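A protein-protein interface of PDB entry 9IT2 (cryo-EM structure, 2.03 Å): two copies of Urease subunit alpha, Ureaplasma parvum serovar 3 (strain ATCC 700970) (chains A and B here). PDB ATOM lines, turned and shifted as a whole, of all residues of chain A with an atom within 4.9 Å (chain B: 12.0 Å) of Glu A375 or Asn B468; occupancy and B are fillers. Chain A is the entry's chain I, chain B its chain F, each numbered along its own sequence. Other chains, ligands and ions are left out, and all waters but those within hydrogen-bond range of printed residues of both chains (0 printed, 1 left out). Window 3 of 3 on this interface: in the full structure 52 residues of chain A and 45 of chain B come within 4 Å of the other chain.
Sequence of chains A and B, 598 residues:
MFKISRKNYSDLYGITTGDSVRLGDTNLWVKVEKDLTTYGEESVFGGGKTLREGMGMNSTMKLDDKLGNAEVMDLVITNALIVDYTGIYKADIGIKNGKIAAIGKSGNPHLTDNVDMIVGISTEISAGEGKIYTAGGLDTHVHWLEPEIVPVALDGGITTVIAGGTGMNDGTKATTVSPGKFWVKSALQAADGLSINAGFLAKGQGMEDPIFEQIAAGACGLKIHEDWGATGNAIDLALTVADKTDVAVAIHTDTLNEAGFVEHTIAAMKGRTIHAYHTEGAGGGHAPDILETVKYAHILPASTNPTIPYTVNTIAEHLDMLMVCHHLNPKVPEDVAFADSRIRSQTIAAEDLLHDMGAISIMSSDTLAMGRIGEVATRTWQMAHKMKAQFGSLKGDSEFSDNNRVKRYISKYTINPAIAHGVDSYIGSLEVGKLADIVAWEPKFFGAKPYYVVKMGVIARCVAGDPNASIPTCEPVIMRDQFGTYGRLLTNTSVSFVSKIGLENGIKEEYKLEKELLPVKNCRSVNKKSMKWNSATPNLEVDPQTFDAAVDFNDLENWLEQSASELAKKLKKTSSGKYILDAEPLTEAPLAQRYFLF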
ATOM      1  N   VAL A 152      -9.227  27.407 -23.221  1.00  0.00           N
ATOM      2  CA  VAL A 152      -9.524  26.295 -22.323  1.00  0.00           C
ATOM      3  C   VAL A 152      -8.289  25.920 -21.513  1.00  0.00           C
ATOM      4  O   VAL A 152      -8.373  25.654 -20.308  1.00  0.00           O
ATOM      5  CB  VAL A 152     -10.066  25.094 -23.117  1.00  0.00           C
ATOM      6  CG1 VAL A 152     -10.238  23.885 -22.207  1.00  0.00           C
ATOM      7  CG2 VAL A 152     -11.384  25.453 -23.777  1.00  0.00           C
ATOM      8  N   ASN A 305      -4.333  12.373 -19.208  1.00  0.00           N
ATOM      9  CA  ASN A 305      -5.335  12.504 -18.151  1.00  0.00           C
ATOM     10  C   ASN A 305      -6.597  11.634 -18.257  1.00  0.00           C
ATOM     11  O   ASN A 305      -7.230  11.417 -17.216  1.00  0.00           O
ATOM     12  CB  ASN A 305      -5.712  13.985 -17.965  1.00  0.00           C
ATOM     13  CG  ASN A 305      -6.297  14.641 -19.210  1.00  0.00           C
ATOM     14  OD1 ASN A 305      -6.945  14.008 -20.032  1.00  0.00           O
ATOM     15  ND2 ASN A 305      -6.067  15.943 -19.338  1.00  0.00           N
ATOM     16  N   GLY A 371      -7.822  12.923 -24.686  1.00  0.00           N
ATOM     17  CA  GLY A 371      -7.963  13.550 -23.387  1.00  0.00           C
ATOM     18  C   GLY A 371      -8.349  15.015 -23.413  1.00  0.00           C
ATOM     19  O   GLY A 371      -8.709  15.557 -24.461  1.00  0.00           O
ATOM     20  N   ARG A 372      -8.250  15.671 -22.259  1.00  0.00           N
ATOM     21  CA  ARG A 372      -8.861  16.974 -22.027  1.00  0.00           C
ATOM     22  C   ARG A 372      -7.795  17.979 -21.614  1.00  0.00           C
ATOM     23  O   ARG A 372      -7.107  17.781 -20.607  1.00  0.00           O
ATOM     24  CB  ARG A 372      -9.953  16.852 -20.963  1.00  0.00           C
ATOM     25  CG  ARG A 372     -11.005  15.819 -21.348  1.00  0.00           C
ATOM     26  CD  ARG A 372     -11.701  15.203 -20.156  1.00  0.00           C
ATOM     27  NE  ARG A 372     -12.683  14.216 -20.588  1.00  0.00           N
ATOM     28  CZ  ARG A 372     -12.578  12.911 -20.377  1.00  0.00           C
ATOM     29  NH1 ARG A 372     -11.547  12.397 -19.729  1.00  0.00           N
ATOM     30  NH2 ARG A 372     -13.530  12.102 -20.834  1.00  0.00           N
ATOM     31  N   ILE A 373      -7.668  19.057 -22.391  1.00  0.00           N
ATOM     32  CA  ILE A 373      -6.605  20.032 -22.162  1.00  0.00           C
ATOM     33  C   ILE A 373      -6.879  20.895 -20.931  1.00  0.00           C
ATOM     34  O   ILE A 373      -5.940  21.379 -20.290  1.00  0.00           O
ATOM     35  CB  ILE A 373      -6.399  20.891 -23.423  1.00  0.00           C
ATOM     36  CG1 ILE A 373      -5.078  21.662 -23.344  1.00  0.00           C
ATOM     37  CG2 ILE A 373      -7.574  21.834 -23.646  1.00  0.00           C
ATOM     38  CD1 ILE A 373      -4.726  22.401 -24.615  1.00  0.00           C
ATOM     39  N   GLY A 374      -8.142  21.102 -20.575  1.00  0.00           N
ATOM     40  CA  GLY A 374      -8.467  21.929 -19.434  1.00  0.00           C
ATOM     41  C   GLY A 374      -8.414  21.236 -18.094  1.00  0.00           C
ATOM     42  O   GLY A 374      -8.672  21.873 -17.067  1.00  0.00           O
ATOM     43  N   GLU A 375      -8.083  19.945 -18.064  1.00  0.00           N
ATOM     44  CA  GLU A 375      -8.149  19.150 -16.845  1.00  0.00           C
ATOM     45  C   GLU A 375      -6.817  18.509 -16.478  1.00  0.00           C
ATOM     46  O   GLU A 375      -6.805  17.508 -15.754  1.00  0.00           O
ATOM     47  CB  GLU A 375      -9.229  18.072 -16.986  1.00  0.00           C
ATOM     48  CG  GLU A 375     -10.499  18.572 -17.651  1.00  0.00           C
ATOM     49  CD  GLU A 375     -11.673  17.636 -17.464  1.00  0.00           C
ATOM     50  OE1 GLU A 375     -11.544  16.655 -16.704  1.00  0.00           O
ATOM     51  OE2 GLU A 375     -12.727  17.885 -18.085  1.00  0.00           O
ATOM     52  N   VAL A 376      -5.697  19.048 -16.964  1.00  0.00           N
ATOM     53  CA  VAL A 376      -4.393  18.484 -16.618  1.00  0.00           C
ATOM     54  C   VAL A 376      -4.131  18.633 -15.124  1.00  0.00           C
ATOM     55  O   VAL A 376      -3.775  17.668 -14.438  1.00  0.00           O
ATOM     56  CB  VAL A 376      -3.282  19.147 -17.453  1.00  0.00           C
ATOM     57  CG1 VAL A 376      -1.920  18.592 -17.059  1.00  0.00           C
ATOM     58  CG2 VAL A 376      -3.540  18.951 -18.938  1.00  0.00           C
ATOM     59  N   ALA A 377      -4.310  19.846 -14.598  1.00  0.00           N
ATOM     60  CA  ALA A 377      -4.085  20.073 -13.174  1.00  0.00           C
ATOM     61  C   ALA A 377      -5.162  19.401 -12.332  1.00  0.00           C
ATOM     62  O   ALA A 377      -4.865  18.802 -11.292  1.00  0.00           O
ATOM     63  CB  ALA A 377      -4.026  21.573 -12.882  1.00  0.00           C
ATOM     64  N   THR A 378      -6.418  19.485 -12.771  1.00  0.00           N
ATOM     65  CA  THR A 378      -7.534  18.979 -11.977  1.00  0.00           C
ATOM     66  C   THR A 378      -7.413  17.478 -11.736  1.00  0.00           C
ATOM     67  O   THR A 378      -7.578  17.001 -10.608  1.00  0.00           O
ATOM     68  CB  THR A 378      -8.858  19.308 -12.673  1.00  0.00           C
ATOM     69  OG1 THR A 378      -9.028  20.729 -12.736  1.00  0.00           O
ATOM     70  CG2 THR A 378     -10.028  18.691 -11.921  1.00  0.00           C
ATOM     71  N   ARG A 379      -7.115  16.717 -12.788  1.00  0.00           N
ATOM     72  CA  ARG A 379      -7.039  15.267 -12.641  1.00  0.00           C
ATOM     73  C   ARG A 379      -5.755  14.848 -11.934  1.00  0.00           C
ATOM     74  O   ARG A 379      -5.692  13.766 -11.338  1.00  0.00           O
ATOM     75  CB  ARG A 379      -7.163  14.597 -14.008  1.00  0.00           C
ATOM     76  CG  ARG A 379      -8.555  14.725 -14.604  1.00  0.00           C
ATOM     77  CD  ARG A 379      -8.637  14.135 -15.996  1.00  0.00           C
ATOM     78  NE  ARG A 379     -10.014  14.063 -16.471  1.00  0.00           N
ATOM     79  CZ  ARG A 379     -10.776  12.982 -16.396  1.00  0.00           C
ATOM     80  NH1 ARG A 379     -10.320  11.848 -15.890  1.00  0.00           N
ATOM     81  NH2 ARG A 379     -12.027  13.037 -16.844  1.00  0.00           N
ATOM     82  N   THR A 380      -4.722  15.690 -11.988  1.00  0.00           N
ATOM     83  CA  THR A 380      -3.498  15.412 -11.245  1.00  0.00           C
ATOM     84  C   THR A 380      -3.761  15.406  -9.743  1.00  0.00           C
ATOM     85  O   THR A 380      -3.325  14.501  -9.023  1.00  0.00           O
ATOM     86  CB  THR A 380      -2.423  16.443 -11.598  1.00  0.00           C
ATOM     87  OG1 THR A 380      -2.025  16.278 -12.963  1.00  0.00           O
ATOM     88  CG2 THR A 380      -1.209  16.286 -10.694  1.00  0.00           C
ATOM     89  N   ALA B 464     -16.926  21.703 -35.531  1.00  0.00           N
ATOM     90  CA  ALA B 464     -16.081  21.260 -34.431  1.00  0.00           C
ATOM     91  C   ALA B 464     -16.838  21.455 -33.127  1.00  0.00           C
ATOM     92  O   ALA B 464     -17.766  22.264 -33.042  1.00  0.00           O
ATOM     93  CB  ALA B 464     -14.747  22.014 -34.402  1.00  0.00           C
ATOM     94  N   GLY B 465     -16.426  20.704 -32.110  1.00  0.00           N
ATOM     95  CA  GLY B 465     -17.142  20.702 -30.852  1.00  0.00           C
ATOM     96  C   GLY B 465     -16.376  21.246 -29.665  1.00  0.00           C
ATOM     97  O   GLY B 465     -15.510  22.114 -29.812  1.00  0.00           O
ATOM     98  N   ASP B 466     -16.708  20.741 -28.475  1.00  0.00           N
ATOM     99  CA  ASP B 466     -16.132  21.139 -27.196  1.00  0.00           C
ATOM    100  C   ASP B 466     -14.609  21.059 -27.242  1.00  0.00           C
ATOM    101  O   ASP B 466     -14.047  19.966 -27.386  1.00  0.00           O
ATOM    102  CB  ASP B 466     -16.694  20.255 -26.078  1.00  0.00           C
ATOM    103  CG  ASP B 466     -15.979  20.447 -24.751  1.00  0.00           C
ATOM    104  OD1 ASP B 466     -15.471  21.557 -24.486  1.00  0.00           O
ATOM    105  OD2 ASP B 466     -15.931  19.477 -23.966  1.00  0.00           O
ATOM    106  N   PRO B 467     -13.911  22.193 -27.139  1.00  0.00           N
ATOM    107  CA  PRO B 467     -12.438  22.151 -27.178  1.00  0.00           C
ATOM    108  C   PRO B 467     -11.823  21.386 -26.020  1.00  0.00           C
ATOM    109  O   PRO B 467     -10.703  20.879 -26.151  1.00  0.00           O
ATOM    110  CB  PRO B 467     -12.040  23.635 -27.154  1.00  0.00           C
ATOM    111  CG  PRO B 467     -13.232  24.359 -26.628  1.00  0.00           C
ATOM    112  CD  PRO B 467     -14.438  23.561 -27.003  1.00  0.00           C
ATOM    113  N   ASN B 468     -12.520  21.291 -24.887  1.00  0.00           N
ATOM    114  CA  ASN B 468     -12.018  20.516 -23.760  1.00  0.00           C
ATOM    115  C   ASN B 468     -12.216  19.018 -23.946  1.00  0.00           C
ATOM    116  O   ASN B 468     -11.580  18.232 -23.241  1.00  0.00           O
ATOM    117  CB  ASN B 468     -12.703  20.968 -22.466  1.00  0.00           C
ATOM    118  CG  ASN B 468     -12.147  20.272 -21.235  1.00  0.00           C
ATOM    119  OD1 ASN B 468     -10.970  20.412 -20.908  1.00  0.00           O
ATOM    120  ND2 ASN B 468     -12.994  19.511 -20.553  1.00  0.00           N
ATOM    121  N   ALA B 469     -13.058  18.608 -24.889  1.00  0.00           N
ATOM    122  CA  ALA B 469     -13.427  17.207 -25.002  1.00  0.00           C
ATOM    123  C   ALA B 469     -12.229  16.344 -25.391  1.00  0.00           C
ATOM    124  O   ALA B 469     -11.214  16.825 -25.904  1.00  0.00           O
ATOM    125  CB  ALA B 469     -14.544  17.034 -26.027  1.00  0.00           C
ATOM    126  N   SER B 470     -12.363  15.041 -25.132  1.00  0.00           N
ATOM    127  CA  SER B 470     -11.327  14.089 -25.511  1.00  0.00           C
ATOM    128  C   SER B 470     -11.280  13.857 -27.014  1.00  0.00           C
ATOM    129  O   SER B 470     -10.249  13.412 -27.524  1.00  0.00           O
ATOM    130  CB  SER B 470     -11.543  12.761 -24.783  1.00  0.00           C
ATOM    131  OG  SER B 470     -12.660  12.063 -25.306  1.00  0.00           O
ATOM    132  N   ILE B 471     -12.370  14.130 -27.723  1.00  0.00           N
ATOM    133  CA  ILE B 471     -12.432  13.986 -29.177  1.00  0.00           C
ATOM    134  C   ILE B 471     -13.129  15.206 -29.764  1.00  0.00           C
ATOM    135  O   ILE B 471     -13.898  15.891 -29.076  1.00  0.00           O
ATOM    136  CB  ILE B 471     -13.161  12.689 -29.594  1.00  0.00           C
ATOM    137  CG1 ILE B 471     -14.672  12.846 -29.464  1.00  0.00           C
ATOM    138  CG2 ILE B 471     -12.662  11.484 -28.797  1.00  0.00           C
ATOM    139  CD1 ILE B 471     -15.411  11.583 -29.756  1.00  0.00           C
ATOM    140  N   PRO B 472     -12.865  15.515 -31.049  1.00  0.00           N
ATOM    141  CA  PRO B 472     -13.332  16.797 -31.601  1.00  0.00           C
ATOM    142  C   PRO B 472     -14.764  16.784 -32.118  1.00  0.00           C
ATOM    143  O   PRO B 472     -15.143  17.672 -32.887  1.00  0.00           O
ATOM    144  CB  PRO B 472     -12.342  17.071 -32.745  1.00  0.00           C
ATOM    145  CG  PRO B 472     -11.424  15.870 -32.817  1.00  0.00           C
ATOM    146  CD  PRO B 472     -12.055  14.777 -32.031  1.00  0.00           C
ATOM    147  N   THR B 473     -15.567  15.803 -31.719  1.00  0.00           N
ATOM    148  CA  THR B 473     -16.940  15.676 -32.197  1.00  0.00           C
ATOM    149  C   THR B 473     -17.937  15.670 -31.042  1.00  0.00           C
ATOM    150  O   THR B 473     -18.953  14.974 -31.080  1.00  0.00           O
ATOM    151  CB  THR B 473     -17.105  14.419 -33.048  1.00  0.00           C
ATOM    152  OG1 THR B 473     -16.559  13.294 -32.349  1.00  0.00           O
ATOM    153  CG2 THR B 473     -16.390  14.580 -34.380  1.00  0.00           C
ATOM    154  N   CYS B 474     -17.664  16.448 -30.000  1.00  0.00           N
ATOM    155  CA  CYS B 474     -18.498  16.461 -28.806  1.00  0.00           C
ATOM    156  C   CYS B 474     -19.331  17.734 -28.745  1.00  0.00           C
ATOM    157  O   CYS B 474     -18.866  18.813 -29.120  1.00  0.00           O
ATOM    158  CB  CYS B 474     -17.643  16.335 -27.547  1.00  0.00           C
ATOM    159  SG  CYS B 474     -16.893  14.707 -27.331  1.00  0.00           S
ATOM    160  N   GLU B 475     -20.561  17.598 -28.262  1.00  0.00           N
ATOM    161  CA  GLU B 475     -21.476  18.728 -28.222  1.00  0.00           C
ATOM    162  C   GLU B 475     -20.951  19.797 -27.265  1.00  0.00           C
ATOM    163  O   GLU B 475     -20.346  19.467 -26.238  1.00  0.00           O
ATOM    164  CB  GLU B 475     -22.870  18.267 -27.791  1.00  0.00           C
ATOM    165  CG  GLU B 475     -23.554  17.340 -28.787  1.00  0.00           C
ATOM    166  CD  GLU B 475     -23.604  17.914 -30.190  1.00  0.00           C
ATOM    167  OE1 GLU B 475     -23.853  19.128 -30.332  1.00  0.00           O
ATOM    168  OE2 GLU B 475     -23.393  17.150 -31.154  1.00  0.00           O
ATOM    169  N   PRO B 476     -21.159  21.090 -27.565  1.00  0.00           N
ATOM    170  CA  PRO B 476     -21.892  21.588 -28.734  1.00  0.00           C
ATOM    171  C   PRO B 476     -21.057  21.607 -30.014  1.00  0.00           C
ATOM    172  O   PRO B 476     -20.040  22.293 -30.094  1.00  0.00           O
ATOM    173  CB  PRO B 476     -22.282  23.004 -28.314  1.00  0.00           C
ATOM    174  CG  PRO B 476     -21.192  23.431 -27.395  1.00  0.00           C
ATOM    175  CD  PRO B 476     -20.666  22.188 -26.716  1.00  0.00           C
ATOM    176  N   VAL B 477     -21.504  20.851 -31.011  1.00  0.00           N
ATOM    177  CA  VAL B 477     -20.817  20.751 -32.292  1.00  0.00           C
ATOM    178  C   VAL B 477     -21.371  21.844 -33.200  1.00  0.00           C
ATOM    179  O   VAL B 477     -22.502  21.750 -33.684  1.00  0.00           O
ATOM    180  CB  VAL B 477     -20.994  19.360 -32.910  1.00  0.00           C
ATOM    181  CG1 VAL B 477     -20.484  19.340 -34.329  1.00  0.00           C
ATOM    182  CG2 VAL B 477     -20.278  18.313 -32.069  1.00  0.00           C
ATOM    183  N   ILE B 478     -20.576  22.891 -33.426  1.00  0.00           N
ATOM    184  CA  ILE B 478     -20.996  24.051 -34.201  1.00  0.00           C
ATOM    185  C   ILE B 478     -19.890  24.421 -35.182  1.00  0.00           C
ATOM    186  O   ILE B 478     -18.775  23.902 -35.129  1.00  0.00           O
ATOM    187  CB  ILE B 478     -21.347  25.263 -33.308  1.00  0.00           C
ATOM    188  CG1 ILE B 478     -20.089  25.814 -32.636  1.00  0.00           C
ATOM    189  CG2 ILE B 478     -22.402  24.892 -32.274  1.00  0.00           C
ATOM    190  CD1 ILE B 478     -20.320  27.082 -31.845  1.00  0.00           C
ATOM    191  N   ARG B 480     -17.061  26.655 -36.302  1.00  0.00           N
ATOM    192  CA  ARG B 480     -16.112  27.450 -35.543  1.00  0.00           C
ATOM    193  C   ARG B 480     -14.978  27.918 -36.443  1.00  0.00           C
ATOM    194  O   ARG B 480     -14.599  27.238 -37.406  1.00  0.00           O
ATOM    195  CB  ARG B 480     -15.523  26.658 -34.365  1.00  0.00           C
ATOM    196  CG  ARG B 480     -16.540  26.131 -33.369  1.00  0.00           C
ATOM    197  CD  ARG B 480     -15.845  25.383 -32.241  1.00  0.00           C
ATOM    198  NE  ARG B 480     -16.779  24.686 -31.365  1.00  0.00           N
ATOM    199  CZ  ARG B 480     -17.079  25.072 -30.133  1.00  0.00           C
ATOM    200  NH1 ARG B 480     -16.546  26.159 -29.600  1.00  0.00           N
ATOM    201  NH2 ARG B 480     -17.933  24.347 -29.416  1.00  0.00           N
ATOM    202  N   GLN B 482     -11.156  28.522 -37.335  1.00  0.00           N
ATOM    203  CA  GLN B 482      -9.999  27.661 -37.172  1.00  0.00           C
ATOM    204  C   GLN B 482      -8.717  28.494 -37.207  1.00  0.00           C
ATOM    205  O   GLN B 482      -8.755  29.730 -37.214  1.00  0.00           O
ATOM    206  CB  GLN B 482     -10.020  26.569 -38.242  1.00  0.00           C
ATOM    207  CG  GLN B 482     -11.200  25.622 -38.094  1.00  0.00           C
ATOM    208  CD  GLN B 482     -11.282  25.008 -36.708  1.00  0.00           C
ATOM    209  OE1 GLN B 482     -10.321  24.410 -36.226  1.00  0.00           O
ATOM    210  NE2 GLN B 482     -12.431  25.158 -36.060  1.00  0.00           N
ATOM    211  N   PHE B 483      -7.572  27.806 -37.215  1.00  0.00           N
ATOM    212  CA  PHE B 483      -6.283  28.489 -37.178  1.00  0.00           C
ATOM    213  C   PHE B 483      -6.058  29.382 -38.390  1.00  0.00           C
ATOM    214  O   PHE B 483      -5.244  30.309 -38.319  1.00  0.00           O
ATOM    215  CB  PHE B 483      -5.148  27.469 -37.072  1.00  0.00           C
ATOM    216  CG  PHE B 483      -5.176  26.665 -35.807  1.00  0.00           C
ATOM    217  CD1 PHE B 483      -4.911  27.262 -34.585  1.00  0.00           C
ATOM    218  CD2 PHE B 483      -5.463  25.311 -35.837  1.00  0.00           C
ATOM    219  CE1 PHE B 483      -4.940  26.525 -33.420  1.00  0.00           C
ATOM    220  CE2 PHE B 483      -5.488  24.568 -34.673  1.00  0.00           C
ATOM    221  CZ  PHE B 483      -5.224  25.175 -33.463  1.00  0.00           C
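Of chain B, only Asn B468 (3.0 Å) comes within 4 Å of Glu A375.
Of chain B, only Pro B467 and Asn B468 come within 4 Å of Val A152.
No residue of chain B comes within 4 Å of Asn A305.
Arg A372 touches just one residue of chain B: Asn B468 (3.1 Å).
No residue of chain B comes within 4 Å of Val A376.
Ala A377 touches none of the printed residues of chain B.
Arg A379 touches none of the printed residues of chain B.
Of the printed residues of chain A, Pro B467 touches Val A152.
Printed residues of chain A within 4 Å of Ser B470: Gly A371 (3.2 Å).
Arg B480 touches none of the printed residues of chain A.
Thr B473 touches none of the printed residues of chain A.
The nearest residue of chain B that does not touch Glu A375 is Ala B469 (6.9 Å).
No position is printed for both chains.
Of the 8 pairs that touch across the chains among the printed residues, none has its exchanged pair printed and touching as well.
The side-chain carboxylate (OD1) of Asp B466 lies within hydrogen-bond range of the backbone NH (N) of Asn B468 (3.0 Å).
The side-chain carboxylate (OE1) of Glu A375 lies within salt-bridge range of the guanidinium group (NE) of Arg A379 (3.0 Å).
The side-chain amide nitrogen (ND2) of Asn A305 is in hydrogen-bond range of the backbone carbonyl oxygen (O) of Arg A372.
The backbone NH of Ala B469 sits at hydrogen-bond distance from the side-chain carboxylate of Asp B466 (3.1 Å).
Printed residues of chain A that touch a printed residue of chain B: Val A152, Gly A371, Arg A372, Ile A373, Gly A374 and Glu A375.
Hydrophobic or aromatic side chains of chain A within 4 Å of the printed part of chain B: Val A152.
Along chain A the printed residues that touch a printed residue of chain B span positions 152 to 375.
Of the 18 printed residues of chain B, 4 touch a printed residue of chain A.
Hydrophobic or aromatic side chains of chain B within 4 Å of the printed part of chain A: Pro B467.
Among the printed residues, 8 pairs touch across the chains.
The side-chain carboxylate (OE2) of Glu A375 is in hydrogen-bond range of the side-chain amide nitrogen (ND2) of Asn B468.
O of Gly A371 sits close to O of Ala B469, 3.2 Å away.
N of Gly A374 lies within hydrogen-bond range of OD1 of Asn B468 (2.9 Å).
Pro B467 touches Val A152 (CG to CG2, 3.6 Å).
Asn B468 touches Val A152.
Ser B470 touches Gly A371.
Arg A372 touches Asn B468.
Ile A373 touches Asn B468 (N to OD1, 3.9 Å).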
